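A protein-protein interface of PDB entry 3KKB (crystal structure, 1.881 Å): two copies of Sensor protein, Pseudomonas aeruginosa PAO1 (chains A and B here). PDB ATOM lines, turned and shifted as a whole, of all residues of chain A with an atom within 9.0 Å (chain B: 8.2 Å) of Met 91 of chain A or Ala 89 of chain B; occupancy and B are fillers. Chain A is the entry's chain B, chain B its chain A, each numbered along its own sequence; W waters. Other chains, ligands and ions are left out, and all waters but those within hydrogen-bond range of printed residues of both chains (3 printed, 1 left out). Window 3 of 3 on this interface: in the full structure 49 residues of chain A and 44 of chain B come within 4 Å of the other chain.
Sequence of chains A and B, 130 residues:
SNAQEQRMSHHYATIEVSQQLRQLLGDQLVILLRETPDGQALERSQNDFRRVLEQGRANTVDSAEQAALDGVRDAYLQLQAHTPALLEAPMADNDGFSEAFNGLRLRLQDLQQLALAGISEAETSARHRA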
ATOM      1  N   LEU A  87      37.719  25.706 -15.609  1.00  0.00           N
ATOM      2  CA  LEU A  87      36.454  25.008 -15.445  1.00  0.00           C
ATOM      3  C   LEU A  87      35.318  25.927 -15.889  1.00  0.00           C
ATOM      4  O   LEU A  87      34.496  26.349 -15.071  1.00  0.00           O
ATOM      5  CB  LEU A  87      36.281  24.605 -13.977  1.00  0.00           C
ATOM      6  CG  LEU A  87      37.329  23.632 -13.421  1.00  0.00           C
ATOM      7  CD1 LEU A  87      37.325  23.675 -11.923  1.00  0.00           C
ATOM      8  CD2 LEU A  87      37.130  22.200 -13.928  1.00  0.00           C
ATOM      9  N   GLU A  88      35.284  26.258 -17.179  1.00  0.00           N
ATOM     10  CA  GLU A  88      34.301  27.217 -17.683  1.00  0.00           C
ATOM     11  C   GLU A  88      32.901  26.631 -17.781  1.00  0.00           C
ATOM     12  O   GLU A  88      32.698  25.566 -18.367  1.00  0.00           O
ATOM     13  CB  GLU A  88      34.693  27.768 -19.058  1.00  0.00           C
ATOM     14  CG  GLU A  88      33.690  28.799 -19.579  1.00  0.00           C
ATOM     15  CD  GLU A  88      33.900  29.172 -21.038  1.00  0.00           C
ATOM     16  OE1 GLU A  88      34.780  28.575 -21.696  1.00  0.00           O
ATOM     17  OE2 GLU A  88      33.168  30.064 -21.526  1.00  0.00           O
ATOM     18  N   ALA A  89      31.937  27.346 -17.217  1.00  0.00           N
ATOM     19  CA  ALA A  89      30.531  27.003 -17.376  1.00  0.00           C
ATOM     20  C   ALA A  89      29.909  28.002 -18.344  1.00  0.00           C
ATOM     21  O   ALA A  89      29.630  29.134 -17.963  1.00  0.00           O
ATOM     22  CB  ALA A  89      29.832  27.065 -16.028  1.00  0.00           C
ATOM     23  N   PRO A  90      29.679  27.587 -19.602  1.00  0.00           N
ATOM     24  CA  PRO A  90      29.267  28.516 -20.664  1.00  0.00           C
ATOM     25  C   PRO A  90      28.020  29.329 -20.334  1.00  0.00           C
ATOM     26  O   PRO A  90      27.916  30.472 -20.774  1.00  0.00           O
ATOM     27  CB  PRO A  90      28.968  27.588 -21.845  1.00  0.00           C
ATOM     28  CG  PRO A  90      29.757  26.360 -21.569  1.00  0.00           C
ATOM     29  CD  PRO A  90      29.739  26.198 -20.085  1.00  0.00           C
ATOM     30  N   MET A  91      27.093  28.754 -19.576  1.00  0.00           N
ATOM     31  CA  MET A  91      25.808  29.407 -19.335  1.00  0.00           C
ATOM     32  C   MET A  91      25.709  30.047 -17.957  1.00  0.00           C
ATOM     33  O   MET A  91      24.654  30.563 -17.586  1.00  0.00           O
ATOM     34  CB  MET A  91      24.655  28.413 -19.516  1.00  0.00           C
ATOM     35  CG  MET A  91      24.571  27.800 -20.895  1.00  0.00           C
ATOM     36  SD  MET A  91      24.405  29.170 -22.256  1.00  0.00           S
ATOM     37  CE  MET A  91      22.886  30.146 -21.539  1.00  0.00           C
ATOM     38  N   ALA A  92      26.804  30.018 -17.200  1.00  0.00           N
ATOM     39  CA  ALA A  92      26.781  30.552 -15.837  1.00  0.00           C
ATOM     40  C   ALA A  92      27.869  31.580 -15.590  1.00  0.00           C
ATOM     41  O   ALA A  92      28.876  31.627 -16.300  1.00  0.00           O
ATOM     42  CB  ALA A  92      26.893  29.428 -14.819  1.00  0.00           C
ATOM     43  N   ASP A  93      27.655  32.395 -14.565  1.00  0.00           N
ATOM     44  CA  ASP A  93      28.629  33.384 -14.136  1.00  0.00           C
ATOM     45  C   ASP A  93      29.673  32.652 -13.305  1.00  0.00           C
ATOM     46  O   ASP A  93      29.441  32.354 -12.137  1.00  0.00           O
ATOM     47  CB  ASP A  93      27.917  34.445 -13.290  1.00  0.00           C
ATOM     48  CG  ASP A  93      28.846  35.561 -12.822  1.00  0.00           C
ATOM     49  OD1 ASP A  93      30.074  35.469 -13.016  1.00  0.00           O
ATOM     50  OD2 ASP A  93      28.340  36.540 -12.238  1.00  0.00           O
ATOM     51  N   ASN A  94      30.822  32.343 -13.899  1.00  0.00           N
ATOM     52  CA  ASN A  94      31.855  31.607 -13.156  1.00  0.00           C
ATOM     53  C   ASN A  94      32.379  32.354 -11.937  1.00  0.00           C
ATOM     54  O   ASN A  94      32.508  31.770 -10.866  1.00  0.00           O
ATOM     55  CB  ASN A  94      33.035  31.225 -14.069  1.00  0.00           C
ATOM     56  CG  ASN A  94      32.847  29.873 -14.726  1.00  0.00           C
ATOM     57  OD1 ASN A  94      32.155  29.751 -15.734  1.00  0.00           O
ATOM     58  ND2 ASN A  94      33.473  28.846 -14.157  1.00  0.00           N
ATOM     59  N   LEU B  32      29.137  18.181  -9.919  1.00  0.00           N
ATOM     60  CA  LEU B  32      29.131  19.351 -10.792  1.00  0.00           C
ATOM     61  C   LEU B  32      30.361  19.388 -11.705  1.00  0.00           C
ATOM     62  O   LEU B  32      30.321  19.970 -12.780  1.00  0.00           O
ATOM     63  CB  LEU B  32      29.042  20.636  -9.959  1.00  0.00           C
ATOM     64  CG  LEU B  32      27.655  21.014  -9.424  1.00  0.00           C
ATOM     65  CD1 LEU B  32      27.703  22.227  -8.494  1.00  0.00           C
ATOM     66  CD2 LEU B  32      26.705  21.258 -10.586  1.00  0.00           C
ATOM     67  N   ARG B  34      31.722  16.722 -13.094  1.00  0.00           N
ATOM     68  CA  ARG B  34      31.697  15.638 -14.078  1.00  0.00           C
ATOM     69  C   ARG B  34      31.465  16.136 -15.500  1.00  0.00           C
ATOM     70  O   ARG B  34      30.879  17.205 -15.705  1.00  0.00           O
ATOM     71  CB  ARG B  34      30.625  14.606 -13.714  1.00  0.00           C
ATOM     72  CG  ARG B  34      30.952  13.859 -12.424  1.00  0.00           C
ATOM     73  CD  ARG B  34      29.840  12.924 -12.007  1.00  0.00           C
ATOM     74  NE  ARG B  34      30.085  12.423 -10.659  1.00  0.00           N
ATOM     75  CZ  ARG B  34      29.183  11.797  -9.911  1.00  0.00           C
ATOM     76  NH1 ARG B  34      29.502  11.398  -8.687  1.00  0.00           N
ATOM     77  NH2 ARG B  34      27.959  11.584 -10.382  1.00  0.00           N
ATOM     78  N   GLU B  35      31.917  15.352 -16.480  1.00  0.00           N
ATOM     79  CA  GLU B  35      31.657  15.659 -17.885  1.00  0.00           C
ATOM     80  C   GLU B  35      30.161  15.781 -18.162  1.00  0.00           C
ATOM     81  O   GLU B  35      29.733  16.664 -18.904  1.00  0.00           O
ATOM     82  CB  GLU B  35      32.278  14.600 -18.801  1.00  0.00           C
ATOM     83  CG  GLU B  35      32.077  14.894 -20.280  1.00  0.00           C
ATOM     84  CD  GLU B  35      32.745  13.872 -21.181  1.00  0.00           C
ATOM     85  OE1 GLU B  35      33.351  12.918 -20.651  1.00  0.00           O
ATOM     86  OE2 GLU B  35      32.672  14.030 -22.421  1.00  0.00           O
ATOM     87  N   PRO B  37      27.150  15.936 -15.523  1.00  0.00           N
ATOM     88  CA  PRO B  37      26.641  15.861 -14.143  1.00  0.00           C
ATOM     89  C   PRO B  37      25.217  15.300 -14.070  1.00  0.00           C
ATOM     90  O   PRO B  37      24.355  15.715 -14.840  1.00  0.00           O
ATOM     91  CB  PRO B  37      26.660  17.327 -13.683  1.00  0.00           C
ATOM     92  CG  PRO B  37      27.658  17.996 -14.586  1.00  0.00           C
ATOM     93  CD  PRO B  37      27.493  17.314 -15.911  1.00  0.00           C
ATOM     94  N   HIS B  82      22.920  29.115  -8.449  1.00  0.00           N
ATOM     95  CA  HIS B  82      23.792  28.917  -9.611  1.00  0.00           C
ATOM     96  C   HIS B  82      23.654  27.539 -10.252  1.00  0.00           C
ATOM     97  O   HIS B  82      24.131  27.316 -11.363  1.00  0.00           O
ATOM     98  CB  HIS B  82      25.256  29.138  -9.225  1.00  0.00           C
ATOM     99  CG  HIS B  82      25.570  30.549  -8.844  1.00  0.00           C
ATOM    100  ND1 HIS B  82      26.022  31.482  -9.755  1.00  0.00           N
ATOM    101  CD2 HIS B  82      25.482  31.194  -7.656  1.00  0.00           C
ATOM    102  CE1 HIS B  82      26.203  32.639  -9.141  1.00  0.00           C
ATOM    103  NE2 HIS B  82      25.880  32.493  -7.868  1.00  0.00           N
ATOM    104  N   THR B  83      23.002  26.623  -9.551  1.00  0.00           N
ATOM    105  CA  THR B  83      22.938  25.225  -9.972  1.00  0.00           C
ATOM    106  C   THR B  83      22.404  24.953 -11.380  1.00  0.00           C
ATOM    107  O   THR B  83      23.037  24.227 -12.159  1.00  0.00           O
ATOM    108  CB  THR B  83      22.144  24.379  -8.958  1.00  0.00           C
ATOM    109  OG1 THR B  83      23.031  23.949  -7.929  1.00  0.00           O
ATOM    110  CG2 THR B  83      21.527  23.155  -9.640  1.00  0.00           C
ATOM    111  N   PRO B  84      21.225  25.500 -11.704  1.00  0.00           N
ATOM    112  CA  PRO B  84      20.619  25.182 -12.997  1.00  0.00           C
ATOM    113  C   PRO B  84      21.529  25.538 -14.170  1.00  0.00           C
ATOM    114  O   PRO B  84      21.624  24.766 -15.124  1.00  0.00           O
ATOM    115  CB  PRO B  84      19.353  26.048 -13.010  1.00  0.00           C
ATOM    116  CG  PRO B  84      19.019  26.230 -11.551  1.00  0.00           C
ATOM    117  CD  PRO B  84      20.347  26.346 -10.870  1.00  0.00           C
ATOM    118  N   ALA B  85      22.183  26.691 -14.105  1.00  0.00           N
ATOM    119  CA  ALA B  85      23.032  27.121 -15.211  1.00  0.00           C
ATOM    120  C   ALA B  85      24.238  26.187 -15.365  1.00  0.00           C
ATOM    121  O   ALA B  85      24.660  25.895 -16.479  1.00  0.00           O
ATOM    122  CB  ALA B  85      23.475  28.559 -15.017  1.00  0.00           C
ATOM    123  N   LEU B  86      24.769  25.698 -14.246  1.00  0.00           N
ATOM    124  CA  LEU B  86      25.905  24.772 -14.288  1.00  0.00           C
ATOM    125  C   LEU B  86      25.549  23.433 -14.925  1.00  0.00           C
ATOM    126  O   LEU B  86      26.424  22.731 -15.437  1.00  0.00           O
ATOM    127  CB  LEU B  86      26.459  24.531 -12.887  1.00  0.00           C
ATOM    128  CG  LEU B  86      27.037  25.759 -12.196  1.00  0.00           C
ATOM    129  CD1 LEU B  86      27.344  25.443 -10.741  1.00  0.00           C
ATOM    130  CD2 LEU B  86      28.274  26.237 -12.930  1.00  0.00           C
ATOM    131  N   LEU B  87      24.269  23.073 -14.869  1.00  0.00           N
ATOM    132  CA  LEU B  87      23.819  21.811 -15.444  1.00  0.00           C
ATOM    133  C   LEU B  87      23.503  21.949 -16.932  1.00  0.00           C
ATOM    134  O   LEU B  87      23.555  20.969 -17.671  1.00  0.00           O
ATOM    135  CB  LEU B  87      22.592  21.266 -14.694  1.00  0.00           C
ATOM    136  CG  LEU B  87      22.788  20.831 -13.240  1.00  0.00           C
ATOM    137  CD1 LEU B  87      21.446  20.467 -12.596  1.00  0.00           C
ATOM    138  CD2 LEU B  87      23.756  19.665 -13.186  1.00  0.00           C
ATOM    139  N   GLU B  88      23.178  23.166 -17.365  1.00  0.00           N
ATOM    140  CA  GLU B  88      22.825  23.410 -18.757  1.00  0.00           C
ATOM    141  C   GLU B  88      24.010  23.145 -19.662  1.00  0.00           C
ATOM    142  O   GLU B  88      23.854  22.669 -20.787  1.00  0.00           O
ATOM    143  CB  GLU B  88      22.378  24.857 -18.966  1.00  0.00           C
ATOM    144  CG  GLU B  88      20.988  25.180 -18.467  1.00  0.00           C
ATOM    145  CD  GLU B  88      20.642  26.643 -18.676  1.00  0.00           C
ATOM    146  OE1 GLU B  88      20.549  27.382 -17.671  1.00  0.00           O
ATOM    147  OE2 GLU B  88      20.482  27.054 -19.846  1.00  0.00           O
ATOM    148  N   ALA B  89      25.194  23.489 -19.169  1.00  0.00           N
ATOM    149  CA  ALA B  89      26.415  23.318 -19.935  1.00  0.00           C
ATOM    150  C   ALA B  89      27.565  23.075 -18.964  1.00  0.00           C
ATOM    151  O   ALA B  89      28.045  24.005 -18.296  1.00  0.00           O
ATOM    152  CB  ALA B  89      26.678  24.533 -20.817  1.00  0.00           C
ATOM    153  N   PRO B  90      28.002  21.813 -18.874  1.00  0.00           N
ATOM    154  CA  PRO B  90      29.021  21.335 -17.925  1.00  0.00           C
ATOM    155  C   PRO B  90      30.346  22.101 -17.984  1.00  0.00           C
ATOM    156  O   PRO B  90      30.769  22.541 -19.062  1.00  0.00           O
ATOM    157  CB  PRO B  90      29.251  19.879 -18.359  1.00  0.00           C
ATOM    158  CG  PRO B  90      28.671  19.783 -19.747  1.00  0.00           C
ATOM    159  CD  PRO B  90      27.520  20.734 -19.748  1.00  0.00           C
ATOM    160  N   MET B  91      30.992  22.227 -16.826  1.00  0.00           N
ATOM    161  CA  MET B  91      32.286  22.895 -16.701  1.00  0.00           C
ATOM    162  C   MET B  91      33.429  22.064 -17.265  1.00  0.00           C
ATOM    163  O   MET B  91      34.351  22.600 -17.874  1.00  0.00           O
ATOM    164  CB  MET B  91      32.592  23.195 -15.232  1.00  0.00           C
ATOM    165  CG  MET B  91      31.793  24.336 -14.636  1.00  0.00           C
ATOM    166  SD  MET B  91      32.307  24.691 -12.795  1.00  0.00           S
ATOM    167  CE  MET B  91      31.171  23.433 -11.833  1.00  0.00           C
ATOM    168  N   ALA B  92      33.368  20.754 -17.050  1.00  0.00           N
ATOM    169  CA  ALA B  92      34.488  19.879 -17.380  1.00  0.00           C
ATOM    170  C   ALA B  92      34.321  19.181 -18.725  1.00  0.00           C
ATOM    171  O   ALA B  92      33.204  19.019 -19.219  1.00  0.00           O
ATOM    172  CB  ALA B  92      34.708  18.861 -16.267  1.00  0.00           C
HETATM  173  O   HOH W   1      26.914  26.399 -17.939  1.00  0.00           O
HETATM  174  O   HOH W   2      24.950  31.845 -12.896  1.00  0.00           O
HETATM  175  O   HOH W   3      36.374  24.721 -19.276  1.00  0.00           O
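The backbone carbonyl oxygen (O) of Met 91 of chain B sits close to the backbone carbonyl oxygen (O) of Glu 88 of chain A, at 3.4 Å. SD of Met 91 of chain B lies close to O of Leu 87 of chain A (3.6 Å).
ND2 of Asn 94 of chain A is in hydrogen-bond range of O of Leu 87 of chain A. N of Ala 89 of chain A lies within hydrogen-bond range of OD1 of Asn 94 of chain A, at 2.8 Å.
Among the printed residues, pairs that only touch across the chains: Pro 90 of chain A with Ala 89 of chain B (3.3 Å), Met 91 of chain A with Ala 85 of chain B (3.5 Å), Ala 92 of chain A with Ala 85 of chain B (3.5 Å), Ala 89 of chain A with Leu 86 of chain B (3.6 Å), Ala 89 of chain A with Met 91 of chain B (3.6 Å), Glu 88 of chain A with Pro 90 of chain B (3.7 Å), Met 91 of chain A with Ala 89 of chain B (3.9 Å), Pro 90 of chain A with Pro 90 of chain B (3.9 Å) and Ala 92 of chain A with Leu 86 of chain B (3.96 Å).
Met 91 of chain A touches just these residues of chain B: Ala 85 and Ala 89. Printed residues of chain A within 4 Å of Ala 89 of chain B: Pro 90 (3.3 Å) and Met 91 (3.9 Å). Of the printed residues of chain B, Pro 90 of chain A touches Ala 89 (3.3 Å) and Pro 90 (3.9 Å). Of chain B, only Ala 85 and Leu 86 come within 4 Å of Ala 92 of chain A. No residue of chain A comes within 4 Å of Glu 88 of chain B. Printed residues of chain A within 4 Å of Ala 85 of chain B: Met 91 and Ala 92. Of the printed residues of chain B, Glu 88 of chain A touches Pro 90 and Met 91. Of the printed residues of chain A, Leu 86 of chain B touches Ala 89 (3.6 Å) and Ala 92 (3.96 Å). Leu 32 of chain B touches none of the printed residues of chain A. Asn 94 of chain A touches none of the printed residues of chain B. The nearest residue of chain B that does not touch Met 91 of chain A is Glu 88 of chain B (4.1 Å). The nearest printed residue of chain A that does not touch Ala 89 of chain B is Ala 89 of chain A (4.002 Å). The nearest printed residue of chain B that does not touch Ala 89 of chain A is Ala 89 of chain B (4.002 Å).
Of the 15 printed residues of chain B, 5 touch a printed residue of chain A. Hydrophobic or aromatic side chains of chain B within 4 Å of the printed part of chain A: Ala 85, Leu 86, Ala 89 and Met 91. Hydrophobic or aromatic side chains of chain A within 4 Å of the printed part of chain B: Ala 89, Pro 90, Met 91 and Ala 92. Along chain A the printed residues that touch a printed residue of chain B span positions 87 to 92. Among the printed residues, no Asp or Glu carboxylate lies within 4 Å of a Lys or Arg side-chain nitrogen of the other chain.
Leu 87 of chain A touches Met 91 of chain B, but with the chains exchanged Met 91 of chain A does not touch Leu 87 of chain B (7.1 Å). Glu 88 of chain A touches Met 91 of chain B, but with the chains exchanged Met 91 of chain A does not touch Glu 88 of chain B (4.1 Å). Pro 90 of chain A touches Ala 89 of chain B, but with the chains exchanged Ala 89 of chain A does not touch Pro 90 of chain B (4.8 Å). Pro 90 of chain A touches its own counterpart, Pro 90 of chain B.
Water W1 lies within hydrogen-bond range of the backbone carbonyl oxygen of Ala 89 of chain B (2.7 Å), the backbone carbonyl oxygen of Ala 85 of chain B (2.7 Å) and the backbone NH of Met 91 of chain A (2.9 Å). Water W3 lies within hydrogen-bond range of N of Glu 88 of chain A (2.8 Å) and O of Met 91 of chain B (3.2 Å). Water W2 lies within hydrogen-bond range of N of Asp 93 of chain A (3.2 Å) and ND1 of His 82 of chain B (3.3 Å).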
